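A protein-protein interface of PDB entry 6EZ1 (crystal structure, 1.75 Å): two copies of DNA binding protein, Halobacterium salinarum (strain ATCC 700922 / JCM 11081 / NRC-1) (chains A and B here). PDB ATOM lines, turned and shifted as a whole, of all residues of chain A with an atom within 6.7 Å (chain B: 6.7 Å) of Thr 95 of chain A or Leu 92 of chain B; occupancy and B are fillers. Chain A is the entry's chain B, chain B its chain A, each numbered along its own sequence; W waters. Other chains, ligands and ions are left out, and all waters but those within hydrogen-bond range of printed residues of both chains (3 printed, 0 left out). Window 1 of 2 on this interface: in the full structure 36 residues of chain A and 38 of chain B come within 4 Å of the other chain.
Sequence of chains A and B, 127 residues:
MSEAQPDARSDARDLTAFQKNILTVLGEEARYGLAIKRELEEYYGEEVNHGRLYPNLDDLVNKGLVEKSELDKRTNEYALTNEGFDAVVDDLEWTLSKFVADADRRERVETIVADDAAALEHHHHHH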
ATOM      1  N   ASP A  90     -18.785  -4.939  -6.474  1.00  0.00           N
ATOM      2  CA  ASP A  90     -18.531  -6.269  -7.011  1.00  0.00           C
ATOM      3  C   ASP A  90     -19.836  -6.961  -7.396  1.00  0.00           C
ATOM      4  O   ASP A  90     -19.945  -7.543  -8.479  1.00  0.00           O
ATOM      5  CB  ASP A  90     -17.758  -7.102  -5.989  1.00  0.00           C
ATOM      6  CG  ASP A  90     -17.567  -8.535  -6.431  1.00  0.00           C
ATOM      7  OD1 ASP A  90     -16.857  -8.757  -7.432  1.00  0.00           O
ATOM      8  OD2 ASP A  90     -18.133  -9.443  -5.782  1.00  0.00           O
ATOM      9  N   ASP A  91     -20.831  -6.898  -6.512  1.00  0.00           N
ATOM     10  CA  ASP A  91     -22.111  -7.543  -6.794  1.00  0.00           C
ATOM     11  C   ASP A  91     -22.830  -6.861  -7.951  1.00  0.00           C
ATOM     12  O   ASP A  91     -23.438  -7.532  -8.792  1.00  0.00           O
ATOM     13  CB  ASP A  91     -22.983  -7.527  -5.540  1.00  0.00           C
ATOM     14  CG  ASP A  91     -23.637  -8.865  -5.271  1.00  0.00           C
ATOM     15  OD1 ASP A  91     -22.986  -9.734  -4.655  1.00  0.00           O
ATOM     16  OD2 ASP A  91     -24.799  -9.057  -5.684  1.00  0.00           O
ATOM     17  N   LEU A  92     -22.784  -5.530  -8.004  1.00  0.00           N
ATOM     18  CA  LEU A  92     -23.392  -4.815  -9.118  1.00  0.00           C
ATOM     19  C   LEU A  92     -22.711  -5.176 -10.432  1.00  0.00           C
ATOM     20  O   LEU A  92     -23.382  -5.401 -11.446  1.00  0.00           O
ATOM     21  CB  LEU A  92     -23.321  -3.311  -8.866  1.00  0.00           C
ATOM     22  CG  LEU A  92     -23.946  -2.420  -9.941  1.00  0.00           C
ATOM     23  CD1 LEU A  92     -25.373  -2.847 -10.236  1.00  0.00           C
ATOM     24  CD2 LEU A  92     -23.890  -0.958  -9.512  1.00  0.00           C
ATOM     25  N   GLU A  93     -21.378  -5.247 -10.427  1.00  0.00           N
ATOM     26  CA  GLU A  93     -20.644  -5.616 -11.633  1.00  0.00           C
ATOM     27  C   GLU A  93     -21.056  -6.999 -12.126  1.00  0.00           C
ATOM     28  O   GLU A  93     -21.291  -7.195 -13.325  1.00  0.00           O
ATOM     29  CB  GLU A  93     -19.139  -5.554 -11.361  1.00  0.00           C
ATOM     30  CG  GLU A  93     -18.549  -4.156 -11.500  1.00  0.00           C
ATOM     31  CD  GLU A  93     -17.128  -4.054 -10.979  1.00  0.00           C
ATOM     32  OE1 GLU A  93     -16.646  -5.019 -10.345  1.00  0.00           O
ATOM     33  OE2 GLU A  93     -16.486  -3.006 -11.205  1.00  0.00           O
ATOM     34  N   TRP A  94     -21.160  -7.972 -11.217  1.00  0.00           N
ATOM     35  CA  TRP A  94     -21.561  -9.316 -11.627  1.00  0.00           C
ATOM     36  C   TRP A  94     -22.990  -9.318 -12.155  1.00  0.00           C
ATOM     37  O   TRP A  94     -23.277  -9.911 -13.203  1.00  0.00           O
ATOM     38  CB  TRP A  94     -21.420 -10.304 -10.463  1.00  0.00           C
ATOM     39  CG  TRP A  94     -21.742 -11.727 -10.873  1.00  0.00           C
ATOM     40  CD1 TRP A  94     -20.964 -12.555 -11.629  1.00  0.00           C
ATOM     41  CD2 TRP A  94     -22.927 -12.474 -10.554  1.00  0.00           C
ATOM     42  NE1 TRP A  94     -21.590 -13.767 -11.805  1.00  0.00           N
ATOM     43  CE2 TRP A  94     -22.795 -13.742 -11.155  1.00  0.00           C
ATOM     44  CE3 TRP A  94     -24.087 -12.194  -9.822  1.00  0.00           C
ATOM     45  CZ2 TRP A  94     -23.773 -14.729 -11.045  1.00  0.00           C
ATOM     46  CZ3 TRP A  94     -25.058 -13.178  -9.715  1.00  0.00           C
ATOM     47  CH2 TRP A  94     -24.894 -14.431 -10.324  1.00  0.00           C
ATOM     48  N   THR A  95     -23.903  -8.663 -11.432  1.00  0.00           N
ATOM     49  CA  THR A  95     -25.288  -8.569 -11.879  1.00  0.00           C
ATOM     50  C   THR A  95     -25.372  -7.969 -13.280  1.00  0.00           C
ATOM     51  O   THR A  95     -26.080  -8.488 -14.151  1.00  0.00           O
ATOM     52  CB  THR A  95     -26.099  -7.736 -10.882  1.00  0.00           C
ATOM     53  OG1 THR A  95     -26.237  -8.456  -9.651  1.00  0.00           O
ATOM     54  CG2 THR A  95     -27.480  -7.400 -11.447  1.00  0.00           C
ATOM     55  N   LEU A  96     -24.652  -6.872 -13.518  1.00  0.00           N
ATOM     56  CA  LEU A  96     -24.691  -6.232 -14.826  1.00  0.00           C
ATOM     57  C   LEU A  96     -24.016  -7.079 -15.898  1.00  0.00           C
ATOM     58  O   LEU A  96     -24.418  -7.031 -17.066  1.00  0.00           O
ATOM     59  CB  LEU A  96     -24.031  -4.852 -14.744  1.00  0.00           C
ATOM     60  CG  LEU A  96     -24.820  -3.770 -14.003  1.00  0.00           C
ATOM     61  CD1 LEU A  96     -24.004  -2.500 -13.875  1.00  0.00           C
ATOM     62  CD2 LEU A  96     -26.137  -3.503 -14.727  1.00  0.00           C
ATOM     63  N   SER A  97     -22.992  -7.856 -15.527  1.00  0.00           N
ATOM     64  CA  SER A  97     -22.331  -8.713 -16.504  1.00  0.00           C
ATOM     65  C   SER A  97     -23.293  -9.757 -17.053  1.00  0.00           C
ATOM     66  O   SER A  97     -23.140 -10.206 -18.195  1.00  0.00           O
ATOM     67  CB  SER A  97     -21.109  -9.386 -15.879  1.00  0.00           C
ATOM     68  OG  SER A  97     -21.491 -10.512 -15.107  1.00  0.00           O
ATOM     69  N   LYS A  98     -24.293 -10.143 -16.264  1.00  0.00           N
ATOM     70  CA  LYS A  98     -25.300 -11.094 -16.711  1.00  0.00           C
ATOM     71  C   LYS A  98     -26.484 -10.400 -17.371  1.00  0.00           C
ATOM     72  O   LYS A  98     -27.064 -10.928 -18.326  1.00  0.00           O
ATOM     73  CB  LYS A  98     -25.783 -11.939 -15.529  1.00  0.00           C
ATOM     74  CG  LYS A  98     -24.694 -12.770 -14.871  1.00  0.00           C
ATOM     75  CD  LYS A  98     -24.004 -13.668 -15.885  1.00  0.00           C
ATOM     76  CE  LYS A  98     -23.047 -14.628 -15.203  1.00  0.00           C
ATOM     77  NZ  LYS A  98     -22.383 -15.545 -16.174  1.00  0.00           N
ATOM     78  N   PHE A  99     -26.846  -9.212 -16.891  1.00  0.00           N
ATOM     79  CA  PHE A  99     -28.043  -8.552 -17.396  1.00  0.00           C
ATOM     80  C   PHE A  99     -27.803  -7.886 -18.744  1.00  0.00           C
ATOM     81  O   PHE A  99     -28.679  -7.913 -19.616  1.00  0.00           O
ATOM     82  CB  PHE A  99     -28.539  -7.513 -16.395  1.00  0.00           C
ATOM     83  CG  PHE A  99     -29.883  -6.957 -16.738  1.00  0.00           C
ATOM     84  CD1 PHE A  99     -31.027  -7.630 -16.356  1.00  0.00           C
ATOM     85  CD2 PHE A  99     -30.006  -5.771 -17.443  1.00  0.00           C
ATOM     86  CE1 PHE A  99     -32.271  -7.133 -16.659  1.00  0.00           C
ATOM     87  CE2 PHE A  99     -31.251  -5.267 -17.755  1.00  0.00           C
ATOM     88  CZ  PHE A  99     -32.389  -5.951 -17.361  1.00  0.00           C
ATOM     89  N   VAL A 100     -26.636  -7.271 -18.928  1.00  0.00           N
ATOM     90  CA  VAL A 100     -26.334  -6.557 -20.163  1.00  0.00           C
ATOM     91  C   VAL A 100     -25.942  -7.573 -21.228  1.00  0.00           C
ATOM     92  O   VAL A 100     -24.757  -7.739 -21.542  1.00  0.00           O
ATOM     93  CB  VAL A 100     -25.232  -5.505 -19.944  1.00  0.00           C
ATOM     94  CG1 VAL A 100     -25.002  -4.702 -21.217  1.00  0.00           C
ATOM     95  CG2 VAL A 100     -25.616  -4.586 -18.785  1.00  0.00           C
ATOM     96  N   ARG A 108     -31.855  -0.449 -21.699  1.00  0.00           N
ATOM     97  CA  ARG A 108     -32.687  -0.423 -20.502  1.00  0.00           C
ATOM     98  C   ARG A 108     -31.903   0.110 -19.310  1.00  0.00           C
ATOM     99  O   ARG A 108     -32.374   0.999 -18.591  1.00  0.00           O
ATOM    100  CB  ARG A 108     -33.238  -1.821 -20.201  1.00  0.00           C
ATOM    101  CG  ARG A 108     -34.157  -1.864 -18.979  1.00  0.00           C
ATOM    102  CD  ARG A 108     -34.534  -3.287 -18.571  1.00  0.00           C
ATOM    103  NE  ARG A 108     -35.499  -3.912 -19.471  1.00  0.00           N
ATOM    104  CZ  ARG A 108     -36.815  -3.926 -19.272  1.00  0.00           C
ATOM    105  NH1 ARG A 108     -37.333  -3.340 -18.201  1.00  0.00           N
ATOM    106  NH2 ARG A 108     -37.616  -4.525 -20.143  1.00  0.00           N
ATOM    107  N   VAL A 109     -30.699  -0.423 -19.081  1.00  0.00           N
ATOM    108  CA  VAL A 109     -29.920   0.010 -17.924  1.00  0.00           C
ATOM    109  C   VAL A 109     -29.513   1.470 -18.077  1.00  0.00           C
ATOM    110  O   VAL A 109     -29.556   2.244 -17.112  1.00  0.00           O
ATOM    111  CB  VAL A 109     -28.693  -0.895 -17.715  1.00  0.00           C
ATOM    112  CG1 VAL A 109     -27.919  -0.439 -16.481  1.00  0.00           C
ATOM    113  CG2 VAL A 109     -29.112  -2.348 -17.576  1.00  0.00           C
ATOM    114  N   ILE A 112     -32.474   3.391 -16.937  1.00  0.00           N
ATOM    115  CA  ILE A 112     -32.646   3.363 -15.490  1.00  0.00           C
ATOM    116  C   ILE A 112     -31.706   4.366 -14.833  1.00  0.00           C
ATOM    117  O   ILE A 112     -32.112   5.168 -13.981  1.00  0.00           O
ATOM    118  CB  ILE A 112     -32.409   1.942 -14.945  1.00  0.00           C
ATOM    119  CG1 ILE A 112     -33.490   0.984 -15.454  1.00  0.00           C
ATOM    120  CG2 ILE A 112     -32.360   1.963 -13.418  1.00  0.00           C
ATOM    121  CD1 ILE A 112     -33.145  -0.482 -15.233  1.00  0.00           C
ATOM    122  N   ASP A 116     -32.642   7.763 -12.823  1.00  0.00           N
ATOM    123  CA  ASP A 116     -32.221   7.909 -11.433  1.00  0.00           C
ATOM    124  C   ASP A 116     -31.377   9.165 -11.246  1.00  0.00           C
ATOM    125  O   ASP A 116     -31.524   9.877 -10.245  1.00  0.00           O
ATOM    126  CB  ASP A 116     -31.444   6.674 -10.984  1.00  0.00           C
ATOM    127  CG  ASP A 116     -32.331   5.459 -10.805  1.00  0.00           C
ATOM    128  OD1 ASP A 116     -33.569   5.612 -10.798  1.00  0.00           O
ATOM    129  OD2 ASP A 116     -31.778   4.346 -10.663  1.00  0.00           O
ATOM    130  N   ASN B  21     -29.451 -15.281  -7.233  1.00  0.00           N
ATOM    131  CA  ASN B  21     -28.315 -15.480  -8.125  1.00  0.00           C
ATOM    132  C   ASN B  21     -28.666 -16.434  -9.258  1.00  0.00           C
ATOM    133  O   ASN B  21     -28.198 -16.259 -10.390  1.00  0.00           O
ATOM    134  CB  ASN B  21     -27.115 -15.979  -7.321  1.00  0.00           C
ATOM    135  CG  ASN B  21     -26.511 -14.892  -6.452  1.00  0.00           C
ATOM    136  OD1 ASN B  21     -26.664 -13.703  -6.732  1.00  0.00           O
ATOM    137  ND2 ASN B  21     -25.816 -15.294  -5.397  1.00  0.00           N
ATOM    138  N   THR B  24     -30.399 -14.324 -11.760  1.00  0.00           N
ATOM    139  CA  THR B  24     -29.438 -13.474 -12.456  1.00  0.00           C
ATOM    140  C   THR B  24     -28.739 -14.240 -13.571  1.00  0.00           C
ATOM    141  O   THR B  24     -28.551 -13.719 -14.679  1.00  0.00           O
ATOM    142  CB  THR B  24     -28.406 -12.931 -11.466  1.00  0.00           C
ATOM    143  OG1 THR B  24     -29.054 -12.096 -10.493  1.00  0.00           O
ATOM    144  CG2 THR B  24     -27.321 -12.136 -12.192  1.00  0.00           C
ATOM    145  N   TYR B  43     -19.173 -17.710  -9.626  1.00  0.00           N
ATOM    146  CA  TYR B  43     -19.515 -16.561  -8.794  1.00  0.00           C
ATOM    147  C   TYR B  43     -18.994 -16.736  -7.376  1.00  0.00           C
ATOM    148  O   TYR B  43     -18.296 -15.862  -6.847  1.00  0.00           O
ATOM    149  CB  TYR B  43     -21.029 -16.356  -8.777  1.00  0.00           C
ATOM    150  CG  TYR B  43     -21.466 -15.312  -7.772  1.00  0.00           C
ATOM    151  CD1 TYR B  43     -21.325 -13.960  -8.042  1.00  0.00           C
ATOM    152  CD2 TYR B  43     -22.010 -15.685  -6.551  1.00  0.00           C
ATOM    153  CE1 TYR B  43     -21.719 -13.000  -7.125  1.00  0.00           C
ATOM    154  CE2 TYR B  43     -22.408 -14.735  -5.630  1.00  0.00           C
ATOM    155  CZ  TYR B  43     -22.257 -13.397  -5.919  1.00  0.00           C
ATOM    156  OH  TYR B  43     -22.651 -12.449  -5.000  1.00  0.00           O
ATOM    157  N   ALA B  87     -38.663  -9.925 -11.716  1.00  0.00           N
ATOM    158  CA  ALA B  87     -37.971  -9.976 -10.432  1.00  0.00           C
ATOM    159  C   ALA B  87     -36.522  -9.527 -10.568  1.00  0.00           C
ATOM    160  O   ALA B  87     -35.989  -8.844  -9.682  1.00  0.00           O
ATOM    161  CB  ALA B  87     -38.042 -11.389  -9.854  1.00  0.00           C
ATOM    162  N   VAL B  88     -35.870  -9.902 -11.669  1.00  0.00           N
ATOM    163  CA  VAL B  88     -34.493  -9.479 -11.902  1.00  0.00           C
ATOM    164  C   VAL B  88     -34.435  -7.971 -12.111  1.00  0.00           C
ATOM    165  O   VAL B  88     -33.597  -7.271 -11.530  1.00  0.00           O
ATOM    166  CB  VAL B  88     -33.905 -10.240 -13.105  1.00  0.00           C
ATOM    167  CG1 VAL B  88     -32.525  -9.711 -13.467  1.00  0.00           C
ATOM    168  CG2 VAL B  88     -33.851 -11.739 -12.817  1.00  0.00           C
ATOM    169  N   VAL B  89     -35.337  -7.444 -12.942  1.00  0.00           N
ATOM    170  CA  VAL B  89     -35.355  -6.010 -13.212  1.00  0.00           C
ATOM    171  C   VAL B  89     -35.707  -5.237 -11.950  1.00  0.00           C
ATOM    172  O   VAL B  89     -35.113  -4.193 -11.655  1.00  0.00           O
ATOM    173  CB  VAL B  89     -36.346  -5.694 -14.347  1.00  0.00           C
ATOM    174  CG1 VAL B  89     -36.504  -4.184 -14.511  1.00  0.00           C
ATOM    175  CG2 VAL B  89     -35.908  -6.341 -15.645  1.00  0.00           C
ATOM    176  N   ASP B  90     -36.697  -5.724 -11.199  1.00  0.00           N
ATOM    177  CA  ASP B  90     -37.127  -5.040  -9.984  1.00  0.00           C
ATOM    178  C   ASP B  90     -35.960  -4.842  -9.027  1.00  0.00           C
ATOM    179  O   ASP B  90     -35.760  -3.749  -8.486  1.00  0.00           O
ATOM    180  CB  ASP B  90     -38.250  -5.835  -9.314  1.00  0.00           C
ATOM    181  CG  ASP B  90     -38.618  -5.294  -7.946  1.00  0.00           C
ATOM    182  OD1 ASP B  90     -39.289  -4.246  -7.872  1.00  0.00           O
ATOM    183  OD2 ASP B  90     -38.242  -5.939  -6.945  1.00  0.00           O
ATOM    184  N   ASP B  91     -35.171  -5.892  -8.810  1.00  0.00           N
ATOM    185  CA  ASP B  91     -34.050  -5.782  -7.885  1.00  0.00           C
ATOM    186  C   ASP B  91     -32.946  -4.908  -8.454  1.00  0.00           C
ATOM    187  O   ASP B  91     -32.313  -4.132  -7.724  1.00  0.00           O
ATOM    188  CB  ASP B  91     -33.512  -7.174  -7.561  1.00  0.00           C
ATOM    189  CG  ASP B  91     -33.552  -7.480  -6.087  1.00  0.00           C
ATOM    190  OD1 ASP B  91     -34.609  -7.279  -5.462  1.00  0.00           O
ATOM    191  OD2 ASP B  91     -32.525  -7.932  -5.550  1.00  0.00           O
ATOM    192  N   LEU B  92     -32.686  -5.019  -9.759  1.00  0.00           N
ATOM    193  CA  LEU B  92     -31.679  -4.169 -10.376  1.00  0.00           C
ATOM    194  C   LEU B  92     -32.065  -2.701 -10.259  1.00  0.00           C
ATOM    195  O   LEU B  92     -31.215  -1.847  -9.977  1.00  0.00           O
ATOM    196  CB  LEU B  92     -31.486  -4.555 -11.840  1.00  0.00           C
ATOM    197  CG  LEU B  92     -30.451  -3.731 -12.606  1.00  0.00           C
ATOM    198  CD1 LEU B  92     -29.078  -3.831 -11.968  1.00  0.00           C
ATOM    199  CD2 LEU B  92     -30.403  -4.177 -14.068  1.00  0.00           C
ATOM    200  N   GLU B  93     -33.348  -2.393 -10.467  1.00  0.00           N
ATOM    201  CA  GLU B  93     -33.810  -1.017 -10.332  1.00  0.00           C
ATOM    202  C   GLU B  93     -33.645  -0.518  -8.901  1.00  0.00           C
ATOM    203  O   GLU B  93     -33.213   0.618  -8.681  1.00  0.00           O
ATOM    204  CB  GLU B  93     -35.266  -0.905 -10.775  1.00  0.00           C
ATOM    205  CG  GLU B  93     -35.476  -1.077 -12.274  1.00  0.00           C
ATOM    206  CD  GLU B  93     -36.940  -1.086 -12.678  1.00  0.00           C
ATOM    207  OE1 GLU B  93     -37.804  -1.415 -11.836  1.00  0.00           O
ATOM    208  OE2 GLU B  93     -37.235  -0.761 -13.846  1.00  0.00           O
ATOM    209  N   TRP B  94     -33.990  -1.343  -7.909  1.00  0.00           N
ATOM    210  CA  TRP B  94     -33.805  -0.915  -6.527  1.00  0.00           C
ATOM    211  C   TRP B  94     -32.326  -0.713  -6.218  1.00  0.00           C
ATOM    212  O   TRP B  94     -31.942   0.288  -5.606  1.00  0.00           O
ATOM    213  CB  TRP B  94     -34.422  -1.924  -5.554  1.00  0.00           C
ATOM    214  CG  TRP B  94     -34.321  -1.460  -4.120  1.00  0.00           C
ATOM    215  CD1 TRP B  94     -35.045  -0.469  -3.528  1.00  0.00           C
ATOM    216  CD2 TRP B  94     -33.432  -1.963  -3.115  1.00  0.00           C
ATOM    217  NE1 TRP B  94     -34.664  -0.321  -2.214  1.00  0.00           N
ATOM    218  CE2 TRP B  94     -33.678  -1.230  -1.936  1.00  0.00           C
ATOM    219  CE3 TRP B  94     -32.456  -2.966  -3.095  1.00  0.00           C
ATOM    220  CZ2 TRP B  94     -32.982  -1.464  -0.753  1.00  0.00           C
ATOM    221  CZ3 TRP B  94     -31.769  -3.195  -1.919  1.00  0.00           C
ATOM    222  CH2 TRP B  94     -32.034  -2.450  -0.766  1.00  0.00           C
ATOM    223  N   THR B  95     -31.482  -1.656  -6.640  1.00  0.00           N
ATOM    224  CA  THR B  95     -30.048  -1.541  -6.395  1.00  0.00           C
ATOM    225  C   THR B  95     -29.485  -0.271  -7.023  1.00  0.00           C
ATOM    226  O   THR B  95     -28.721   0.466  -6.385  1.00  0.00           O
ATOM    227  CB  THR B  95     -29.328  -2.778  -6.934  1.00  0.00           C
ATOM    228  OG1 THR B  95     -29.712  -3.931  -6.171  1.00  0.00           O
ATOM    229  CG2 THR B  95     -27.816  -2.598  -6.869  1.00  0.00           C
ATOM    230  N   LEU B  96     -29.853   0.004  -8.276  1.00  0.00           N
ATOM    231  CA  LEU B  96     -29.357   1.204  -8.940  1.00  0.00           C
ATOM    232  C   LEU B  96     -29.934   2.474  -8.323  1.00  0.00           C
ATOM    233  O   LEU B  96     -29.250   3.504  -8.286  1.00  0.00           O
ATOM    234  CB  LEU B  96     -29.676   1.147 -10.435  1.00  0.00           C
ATOM    235  CG  LEU B  96     -28.904   0.097 -11.240  1.00  0.00           C
ATOM    236  CD1 LEU B  96     -29.455  -0.028 -12.649  1.00  0.00           C
ATOM    237  CD2 LEU B  96     -27.420   0.449 -11.273  1.00  0.00           C
ATOM    238  N   SER B  97     -31.181   2.433  -7.846  1.00  0.00           N
ATOM    239  CA  SER B  97     -31.752   3.607  -7.192  1.00  0.00           C
ATOM    240  C   SER B  97     -30.922   4.002  -5.977  1.00  0.00           C
ATOM    241  O   SER B  97     -30.762   5.193  -5.682  1.00  0.00           O
ATOM    242  CB  SER B  97     -33.207   3.333  -6.803  1.00  0.00           C
ATOM    243  OG  SER B  97     -33.292   2.583  -5.601  1.00  0.00           O
ATOM    244  N   ASP B 116     -19.419  -3.851 -20.686  1.00  0.00           N
ATOM    245  CA  ASP B 116     -20.083  -5.138 -20.865  1.00  0.00           C
ATOM    246  C   ASP B 116     -20.668  -5.263 -22.265  1.00  0.00           C
ATOM    247  O   ASP B 116     -20.524  -6.305 -22.917  1.00  0.00           O
ATOM    248  CB  ASP B 116     -21.180  -5.322 -19.815  1.00  0.00           C
ATOM    249  CG  ASP B 116     -20.625  -5.545 -18.418  1.00  0.00           C
ATOM    250  OD1 ASP B 116     -19.434  -5.898 -18.296  1.00  0.00           O
ATOM    251  OD2 ASP B 116     -21.392  -5.376 -17.446  1.00  0.00           O
HETATM  252  O   HOH W   1     -19.854  -6.010 -15.369  1.00  0.00           O
HETATM  253  O   HOH W   2     -33.641   2.669 -10.329  1.00  0.00           O
HETATM  254  O   HOH W   3     -36.315  -1.091 -16.396  1.00  0.00           O
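OH of Tyr 43 of chain B lies within hydrogen-bond range of OD1 of Asp 91 of chain A (2.8 Å). N of Ser 97 of chain B is in hydrogen-bond range of OD2 of Asp 116 of chain A (3.5 Å). O of Leu 96 of chain A sits close to OD2 of Asp 116 of chain B, 3.5 Å away.
O of Trp 94 of chain B lies within hydrogen-bond range of OG of Ser 97 of chain B (2.7 Å). OG1 of Thr 95 of chain A is in hydrogen-bond range of O of Asp 91 of chain A, at 3.1 Å. O of Trp 94 of chain A is in hydrogen-bond range of OG of Ser 97 of chain A (2.7 Å).
Among the printed residues, pairs that only touch across the chains: Trp 94 of chain A with Asn 21 of chain B (3.4 Å), Trp 94 of chain A with Thr 24 of chain B (3.5 Å), Trp 94 of chain A with Tyr 43 of chain B (3.3 Å), Thr 95 of chain A with Leu 92 of chain B (3.9 Å), Ser 97 of chain A with Asp 116 of chain B (3.5 Å), Lys 98 of chain A with Thr 24 of chain B (3.4 Å), Phe 99 of chain A with Val 88 of chain B (3.9 Å), Phe 99 of chain A with Val 89 of chain B (3.9 Å), Phe 99 of chain A with Leu 92 of chain B (3.8 Å), Arg 108 of chain A with Val 89 of chain B (3.9 Å), Ile 112 of chain A with Glu 93 of chain B (3.8 Å), Ile 112 of chain A with Leu 96 of chain B (3.6 Å) and Asp 116 of chain A with Leu 96 of chain B (3.5 Å).
Of chain B, only Leu 92 (3.9 Å) comes within 4 Å of Thr 95 of chain A. Leu 92 of chain B touches two residues of chain A. Printed residues of chain B within 4 Å of Arg 108 of chain A: Val 89. Of the printed residues of chain A, Asn 21 of chain B touches Trp 94. Of the printed residues of chain A, Leu 96 of chain B touches Ile 112 and Asp 116. Of the printed residues of chain A, Ser 97 of chain B touches Asp 116.
Of the 15 printed residues of chain B, 10 touch a printed residue of chain A. Of the 15 printed residues of chain A, 10 touch a printed residue of chain B. Hydrophobic or aromatic side chains of chain A that line the printed part of chain B: Trp 94, Leu 96, Phe 99 and Ile 112. Along chain A the printed residues that touch a printed residue of chain B span positions 91 to 116. Among the printed residues, no Asp or Glu carboxylate lies within 4 Å of a Lys or Arg side-chain nitrogen of the other chain.
Thr 95 of chain A touches Leu 92 of chain B, but with the chains exchanged Leu 92 of chain A does not touch Thr 95 of chain B (4.2 Å). Leu 96 of chain A touches Asp 116 of chain B, and with the chains exchanged Asp 116 of chain A touches Leu 96 of chain B. Ser 97 of chain A touches Asp 116 of chain B, and with the chains exchanged Asp 116 of chain A touches Ser 97 of chain B. Positions printed for both chains: 90, 91, 92, 93, 94, 95, 96, 97 and 116. Of the 16 pairs that touch across the chains among the printed residues, 4 have their exchanged pair printed and touching as well.
Water W2 bridges the side-chain carboxylate of Asp 116 of chain A and the backbone carbonyl oxygen of Glu 93 of chain B. Water W1 lies within hydrogen-bond range of the side-chain carboxylate (OD2) of Asp 116 of chain B (2.7 Å) and the backbone carbonyl oxygen (O) of Glu 93 of chain A (2.8 Å). Water W3 bridges OE2 of Glu 93 of chain B (2.7 Å) and NH1 of Arg 108 of chain A (3.1 Å).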
